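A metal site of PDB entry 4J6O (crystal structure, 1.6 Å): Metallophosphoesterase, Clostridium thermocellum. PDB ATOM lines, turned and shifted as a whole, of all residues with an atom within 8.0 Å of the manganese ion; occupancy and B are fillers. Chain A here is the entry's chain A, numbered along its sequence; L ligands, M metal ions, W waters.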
ATOM      1  N   GLY A  18      26.272 -16.577   8.666  1.00  0.00           N
ATOM      2  CA  GLY A  18      25.443 -17.482   7.865  1.00  0.00           C
ATOM      3  C   GLY A  18      26.259 -18.414   6.995  1.00  0.00           C
ATOM      4  O   GLY A  18      27.456 -18.613   7.171  1.00  0.00           O
ATOM      5  N   ASP A  19      25.569 -19.073   6.056  1.00  0.00           N
ATOM      6  CA  ASP A  19      26.195 -20.162   5.302  1.00  0.00           C
ATOM      7  C   ASP A  19      27.429 -19.716   4.537  1.00  0.00           C
ATOM      8  O   ASP A  19      27.374 -18.798   3.704  1.00  0.00           O
ATOM      9  CB  ASP A  19      25.200 -20.667   4.254  1.00  0.00           C
ATOM     10  CG  ASP A  19      23.874 -21.072   4.823  1.00  0.00           C
ATOM     11  OD1 ASP A  19      23.232 -20.376   5.663  1.00  0.00           O
ATOM     12  OD2 ASP A  19      23.378 -22.142   4.323  1.00  0.00           O
ATOM     13  N   ILE A  20      28.499 -20.455   4.762  1.00  0.00           N
ATOM     14  CA  ILE A  20      29.772 -20.154   4.160  1.00  0.00           C
ATOM     15  C   ILE A  20      30.034 -20.927   2.868  1.00  0.00           C
ATOM     16  O   ILE A  20      30.557 -20.338   1.927  1.00  0.00           O
ATOM     17  CB  ILE A  20      30.882 -20.388   5.184  1.00  0.00           C
ATOM     18  CG1 ILE A  20      30.688 -19.418   6.385  1.00  0.00           C
ATOM     19  CG2 ILE A  20      32.260 -20.236   4.552  1.00  0.00           C
ATOM     20  CD1 ILE A  20      31.427 -19.865   7.677  1.00  0.00           C
ATOM     21  N   HIS A  21      29.609 -22.224   2.855  1.00  0.00           N
ATOM     22  CA  HIS A  21      29.713 -23.027   1.625  1.00  0.00           C
ATOM     23  C   HIS A  21      31.073 -22.790   0.923  1.00  0.00           C
ATOM     24  O   HIS A  21      31.143 -22.460  -0.274  1.00  0.00           O
ATOM     25  CB  HIS A  21      28.549 -22.689   0.685  1.00  0.00           C
ATOM     26  CG  HIS A  21      27.245 -23.271   1.128  1.00  0.00           C
ATOM     27  ND1 HIS A  21      27.094 -24.615   1.363  1.00  0.00           N
ATOM     28  CD2 HIS A  21      26.041 -22.702   1.351  1.00  0.00           C
ATOM     29  CE1 HIS A  21      25.865 -24.847   1.762  1.00  0.00           C
ATOM     30  NE2 HIS A  21      25.199 -23.706   1.750  1.00  0.00           N
ATOM     31  N   LEU A  63      26.434 -20.727  11.731  1.00  0.00           N
ATOM     32  CA  LEU A  63      25.095 -21.318  11.523  1.00  0.00           C
ATOM     33  C   LEU A  63      25.161 -22.567  10.665  1.00  0.00           C
ATOM     34  O   LEU A  63      24.112 -23.193  10.358  1.00  0.00           O
ATOM     35  CB  LEU A  63      24.147 -20.304  10.942  1.00  0.00           C
ATOM     36  CG  LEU A  63      23.866 -19.102  11.825  1.00  0.00           C
ATOM     37  CD1 LEU A  63      22.822 -18.209  11.130  1.00  0.00           C
ATOM     38  CD2 LEU A  63      23.315 -19.584  13.170  1.00  0.00           C
ATOM     39  N   GLY A  64      26.378 -22.974  10.350  1.00  0.00           N
ATOM     40  CA  GLY A  64      26.617 -24.218   9.637  1.00  0.00           C
ATOM     41  C   GLY A  64      26.553 -24.059   8.129  1.00  0.00           C
ATOM     42  O   GLY A  64      26.592 -22.925   7.597  1.00  0.00           O
ATOM     43  N   ASP A  65      26.453 -25.163   7.424  1.00  0.00           N
ATOM     44  CA  ASP A  65      26.597 -25.232   5.943  1.00  0.00           C
ATOM     45  C   ASP A  65      27.964 -24.637   5.568  1.00  0.00           C
ATOM     46  O   ASP A  65      28.086 -23.693   4.768  1.00  0.00           O
ATOM     47  CB  ASP A  65      25.454 -24.554   5.222  1.00  0.00           C
ATOM     48  CG  ASP A  65      24.341 -25.563   4.810  1.00  0.00           C
ATOM     49  OD1 ASP A  65      24.422 -26.696   5.302  1.00  0.00           O
ATOM     50  OD2 ASP A  65      23.418 -25.230   4.050  1.00  0.00           O
ATOM     51  N   LEU A  66      28.993 -25.187   6.211  1.00  0.00           N
ATOM     52  CA  LEU A  66      30.413 -24.829   5.956  1.00  0.00           C
ATOM     53  C   LEU A  66      30.910 -25.400   4.642  1.00  0.00           C
ATOM     54  O   LEU A  66      31.797 -24.812   3.997  1.00  0.00           O
ATOM     55  CB  LEU A  66      31.290 -25.392   7.109  1.00  0.00           C
ATOM     56  CG  LEU A  66      30.854 -25.049   8.513  1.00  0.00           C
ATOM     57  CD1 LEU A  66      31.893 -25.728   9.449  1.00  0.00           C
ATOM     58  CD2 LEU A  66      30.815 -23.540   8.739  1.00  0.00           C
ATOM     59  N   VAL A  67      30.334 -26.550   4.243  1.00  0.00           N
ATOM     60  CA  VAL A  67      30.855 -27.292   3.114  1.00  0.00           C
ATOM     61  C   VAL A  67      29.957 -27.203   1.890  1.00  0.00           C
ATOM     62  O   VAL A  67      28.885 -26.628   1.965  1.00  0.00           O
ATOM     63  CB  VAL A  67      31.059 -28.782   3.525  1.00  0.00           C
ATOM     64  CG1 VAL A  67      31.951 -28.884   4.787  1.00  0.00           C
ATOM     65  CG2 VAL A  67      29.716 -29.432   3.841  1.00  0.00           C
ATOM     66  N   ASP A  68      30.475 -27.700   0.763  1.00  0.00           N
ATOM     67  CA  ASP A  68      29.782 -27.745  -0.546  1.00  0.00           C
ATOM     68  C   ASP A  68      29.855 -26.449  -1.325  1.00  0.00           C
ATOM     69  O   ASP A  68      29.915 -25.364  -0.726  1.00  0.00           O
ATOM     70  CB  ASP A  68      28.321 -28.196  -0.386  1.00  0.00           C
ATOM     71  CG  ASP A  68      28.214 -29.681   0.024  1.00  0.00           C
ATOM     72  OD1 ASP A  68      29.245 -30.338   0.234  1.00  0.00           O
ATOM     73  OD2 ASP A  68      27.073 -30.140   0.183  1.00  0.00           O
ATOM     74  N   ARG A  69      29.946 -26.587  -2.648  1.00  0.00           N
ATOM     75  CA  ARG A  69      29.759 -25.509  -3.643  1.00  0.00           C
ATOM     76  C   ARG A  69      30.975 -24.656  -3.869  1.00  0.00           C
ATOM     77  O   ARG A  69      31.436 -24.486  -4.998  1.00  0.00           O
ATOM     78  CB  ARG A  69      28.587 -24.593  -3.363  1.00  0.00           C
ATOM     79  CG  ARG A  69      27.218 -25.304  -3.425  1.00  0.00           C
ATOM     80  CD  ARG A  69      26.094 -24.308  -3.244  1.00  0.00           C
ATOM     81  NE  ARG A  69      24.770 -24.951  -3.399  1.00  0.00           N
ATOM     82  CZ  ARG A  69      23.912 -25.129  -2.404  1.00  0.00           C
ATOM     83  NH1 ARG A  69      24.230 -24.787  -1.146  1.00  0.00           N
ATOM     84  NH2 ARG A  69      22.724 -25.704  -2.636  1.00  0.00           N
ATOM     85  N   GLY A  94      24.571 -27.501   9.570  1.00  0.00           N
ATOM     86  CA  GLY A  94      23.653 -27.345   8.454  1.00  0.00           C
ATOM     87  C   GLY A  94      23.390 -28.726   7.821  1.00  0.00           C
ATOM     88  O   GLY A  94      24.131 -29.701   8.080  1.00  0.00           O
ATOM     89  N   ASN A  95      22.380 -28.775   6.948  1.00  0.00           N
ATOM     90  CA  ASN A  95      22.041 -29.995   6.260  1.00  0.00           C
ATOM     91  C   ASN A  95      23.212 -30.537   5.435  1.00  0.00           C
ATOM     92  O   ASN A  95      23.422 -31.770   5.324  1.00  0.00           O
ATOM     93  CB  ASN A  95      20.760 -29.773   5.406  1.00  0.00           C
ATOM     94  CG  ASN A  95      20.782 -28.486   4.505  1.00  0.00           C
ATOM     95  OD1 ASN A  95      21.242 -27.340   4.865  1.00  0.00           O
ATOM     96  ND2 ASN A  95      20.237 -28.675   3.308  1.00  0.00           N
ATOM     97  N   HIS A  96      23.962 -29.630   4.811  1.00  0.00           N
ATOM     98  CA  HIS A  96      25.064 -30.081   3.977  1.00  0.00           C
ATOM     99  C   HIS A  96      26.141 -30.714   4.821  1.00  0.00           C
ATOM    100  O   HIS A  96      26.810 -31.661   4.349  1.00  0.00           O
ATOM    101  CB  HIS A  96      25.646 -28.887   3.174  1.00  0.00           C
ATOM    102  CG  HIS A  96      24.735 -28.406   2.085  1.00  0.00           C
ATOM    103  ND1 HIS A  96      24.984 -28.642   0.752  1.00  0.00           N
ATOM    104  CD2 HIS A  96      23.568 -27.709   2.133  1.00  0.00           C
ATOM    105  CE1 HIS A  96      24.011 -28.131   0.032  1.00  0.00           C
ATOM    106  NE2 HIS A  96      23.132 -27.574   0.835  1.00  0.00           N
ATOM    107  N   HIS A 113      24.183 -30.739  -5.257  1.00  0.00           N
ATOM    108  CA  HIS A 113      24.179 -29.428  -4.606  1.00  0.00           C
ATOM    109  C   HIS A 113      25.539 -29.076  -4.079  1.00  0.00           C
ATOM    110  O   HIS A 113      25.620 -28.466  -2.992  1.00  0.00           O
ATOM    111  CB  HIS A 113      23.177 -29.417  -3.472  1.00  0.00           C
ATOM    112  CG  HIS A 113      21.775 -29.656  -3.922  1.00  0.00           C
ATOM    113  ND1 HIS A 113      21.032 -30.736  -3.498  1.00  0.00           N
ATOM    114  CD2 HIS A 113      20.993 -28.966  -4.782  1.00  0.00           C
ATOM    115  CE1 HIS A 113      19.841 -30.688  -4.063  1.00  0.00           C
ATOM    116  NE2 HIS A 113      19.789 -29.627  -4.854  1.00  0.00           N
ATOM    117  N   HIS A 155      20.409 -23.726  12.336  1.00  0.00           N
ATOM    118  CA  HIS A 155      20.565 -23.519  10.880  1.00  0.00           C
ATOM    119  C   HIS A 155      19.250 -23.163  10.210  1.00  0.00           C
ATOM    120  O   HIS A 155      19.155 -22.096   9.557  1.00  0.00           O
ATOM    121  CB  HIS A 155      21.170 -24.771  10.229  1.00  0.00           C
ATOM    122  CG  HIS A 155      21.311 -24.640   8.773  1.00  0.00           C
ATOM    123  ND1 HIS A 155      22.275 -23.834   8.199  1.00  0.00           N
ATOM    124  CD2 HIS A 155      20.597 -25.165   7.764  1.00  0.00           C
ATOM    125  CE1 HIS A 155      22.144 -23.869   6.882  1.00  0.00           C
ATOM    126  NE2 HIS A 155      21.142 -24.682   6.586  1.00  0.00           N
ATOM    127  N   GLY A 207      19.764 -19.430   9.301  1.00  0.00           N
ATOM    128  CA  GLY A 207      20.255 -19.275   7.932  1.00  0.00           C
ATOM    129  C   GLY A 207      19.658 -20.377   7.061  1.00  0.00           C
ATOM    130  O   GLY A 207      20.381 -21.311   6.669  1.00  0.00           O
ATOM    131  N   HIS A 208      18.370 -20.272   6.760  1.00  0.00           N
ATOM    132  CA  HIS A 208      17.725 -21.364   6.050  1.00  0.00           C
ATOM    133  C   HIS A 208      17.786 -21.159   4.555  1.00  0.00           C
ATOM    134  O   HIS A 208      18.854 -21.299   3.985  1.00  0.00           O
ATOM    135  CB  HIS A 208      16.263 -21.560   6.514  1.00  0.00           C
ATOM    136  CG  HIS A 208      15.693 -22.893   6.130  1.00  0.00           C
ATOM    137  ND1 HIS A 208      16.438 -23.926   5.592  1.00  0.00           N
ATOM    138  CD2 HIS A 208      14.427 -23.361   6.271  1.00  0.00           C
ATOM    139  CE1 HIS A 208      15.632 -24.970   5.366  1.00  0.00           C
ATOM    140  NE2 HIS A 208      14.426 -24.654   5.771  1.00  0.00           N
ATOM    141  N   THR A 209      16.674 -20.900   3.884  1.00  0.00           N
ATOM    142  CA  THR A 209      16.802 -20.721   2.439  1.00  0.00           C
ATOM    143  C   THR A 209      17.496 -19.361   2.200  1.00  0.00           C
ATOM    144  O   THR A 209      17.246 -18.355   2.882  1.00  0.00           O
ATOM    145  CB  THR A 209      15.418 -20.832   1.726  1.00  0.00           C
ATOM    146  OG1 THR A 209      14.560 -19.802   2.192  1.00  0.00           O
ATOM    147  CG2 THR A 209      14.802 -22.148   2.057  1.00  0.00           C
ATOM    148  N   PRO A 210      18.386 -19.319   1.218  1.00  0.00           N
ATOM    149  CA  PRO A 210      19.152 -18.090   0.970  1.00  0.00           C
ATOM    150  C   PRO A 210      18.298 -16.931   0.449  1.00  0.00           C
ATOM    151  O   PRO A 210      17.320 -17.130  -0.296  1.00  0.00           O
ATOM    152  CB  PRO A 210      20.217 -18.518  -0.072  1.00  0.00           C
ATOM    153  CG  PRO A 210      19.729 -19.796  -0.611  1.00  0.00           C
ATOM    154  CD  PRO A 210      18.934 -20.465   0.487  1.00  0.00           C
ATOM    155  N   ASP A 224      21.187 -15.893   5.902  1.00  0.00           N
ATOM    156  CA  ASP A 224      21.846 -16.490   4.732  1.00  0.00           C
ATOM    157  C   ASP A 224      21.601 -15.654   3.488  1.00  0.00           C
ATOM    158  O   ASP A 224      20.552 -15.813   2.854  1.00  0.00           O
ATOM    159  CB  ASP A 224      21.319 -17.919   4.500  1.00  0.00           C
ATOM    160  CG  ASP A 224      21.991 -18.596   3.315  1.00  0.00           C
ATOM    161  OD1 ASP A 224      22.893 -17.978   2.748  1.00  0.00           O
ATOM    162  OD2 ASP A 224      21.638 -19.768   2.991  1.00  0.00           O
ATOM    163  N   GLY A 226      23.346 -15.756   0.792  1.00  0.00           N
ATOM    164  CA  GLY A 226      23.789 -16.478  -0.389  1.00  0.00           C
ATOM    165  C   GLY A 226      25.154 -16.103  -0.930  1.00  0.00           C
ATOM    166  O   GLY A 226      25.349 -15.936  -2.142  1.00  0.00           O
ATOM    167  N   VAL A 228      27.845 -17.849  -1.516  1.00  0.00           N
ATOM    168  CA  VAL A 228      28.414 -18.654  -2.577  1.00  0.00           C
ATOM    169  C   VAL A 228      27.756 -18.521  -3.951  1.00  0.00           C
ATOM    170  O   VAL A 228      28.389 -18.810  -4.968  1.00  0.00           O
ATOM    171  CB  VAL A 228      28.444 -20.145  -2.124  1.00  0.00           C
ATOM    172  CG1 VAL A 228      27.021 -20.771  -2.167  1.00  0.00           C
ATOM    173  CG2 VAL A 228      29.427 -20.969  -2.978  1.00  0.00           C
ATOM    174  N   PHE A 229      26.526 -17.986  -3.950  1.00  0.00           N
ATOM    175  CA  PHE A 229      25.755 -17.744  -5.168  1.00  0.00           C
ATOM    176  C   PHE A 229      26.038 -16.378  -5.775  1.00  0.00           C
ATOM    177  O   PHE A 229      25.309 -15.934  -6.661  1.00  0.00           O
ATOM    178  CB  PHE A 229      24.268 -17.888  -4.855  1.00  0.00           C
ATOM    179  CG  PHE A 229      23.920 -19.195  -4.240  1.00  0.00           C
ATOM    180  CD1 PHE A 229      24.128 -20.365  -4.960  1.00  0.00           C
ATOM    181  CD2 PHE A 229      23.435 -19.292  -2.933  1.00  0.00           C
ATOM    182  CE1 PHE A 229      23.782 -21.610  -4.383  1.00  0.00           C
ATOM    183  CE2 PHE A 229      23.100 -20.552  -2.330  1.00  0.00           C
ATOM    184  CZ  PHE A 229      23.290 -21.719  -3.093  1.00  0.00           C
HETATM  185  C1  LIG L   1      19.880 -24.272   3.363  1.00  0.00           C
HETATM  186  O1  LIG L   1      20.931 -23.529   3.393  1.00  0.00           O
HETATM  187  O2  LIG L   1      19.524 -24.759   4.472  1.00  0.00           O
HETATM  188  C2  LIG L   1      19.130 -24.532   2.070  1.00  0.00           C
HETATM  189  C3  LIG L   1      19.993 -25.297   1.063  1.00  0.00           C
HETATM  190  O3  LIG L   1      20.481 -26.452   1.828  1.00  0.00           O
HETATM  191  C4  LIG L   1      18.864 -25.637   0.087  1.00  0.00           C
HETATM  192  C5  LIG L   1      19.807 -26.491  -0.711  1.00  0.00           C
HETATM  193  O4  LIG L   1      20.981 -26.895  -0.880  1.00  0.00           O
HETATM  194  O5  LIG L   1      19.130 -27.017  -1.646  1.00  0.00           O
HETATM  195  C6  LIG L   1      21.196 -24.439   0.619  1.00  0.00           C
HETATM  196  O6  LIG L   1      22.312 -24.773   1.081  1.00  0.00           O
HETATM  197  O7  LIG L   1      20.894 -23.430  -0.102  1.00  0.00           O
HETATM  198 MN    MN M   1      23.129 -23.565   2.713  1.00  0.00          MN
HETATM  199  O   HOH W   1      22.637 -21.724   1.412  1.00  0.00           O
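The manganese ion is bound by the side-chain carboxylate of Asp 65 (2.2 Å), the side-chain carboxylate of Asp 19 (2.2 Å), an oxygen (O6) of the ligand (2.2 Å), a ring nitrogen (NE2) of His 21 (2.3 Å), an oxygen (O1) of the ligand (2.3 Å) and water W1 (2.3 Å).
The side-chain amide oxygen (OD1) of Asn 95 sits close to the side-chain carboxylate (OD1) of Asp 65, at 3.3 Å. The backbone NH (N) of His 96 lies within hydrogen-bond range of the side-chain carboxylate (OD1) of Asp 65 (3.0 Å). O of Asp 65 is in hydrogen-bond range of N of Ile 20, at 3.3 Å. A ring nitrogen (NE2) of His 21 sits close to the guanidinium group (NH1) of Arg 69 (3.2 Å). A ring nitrogen (ND1) of His 21 lies within hydrogen-bond range of the backbone carbonyl oxygen (O) of Val 67. OD2 of Asp 65 sits close to NE2 of His 155.
Three residues have an atom within 4 Å of the manganese ion: Asp 19, His 21 and Asp 65.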
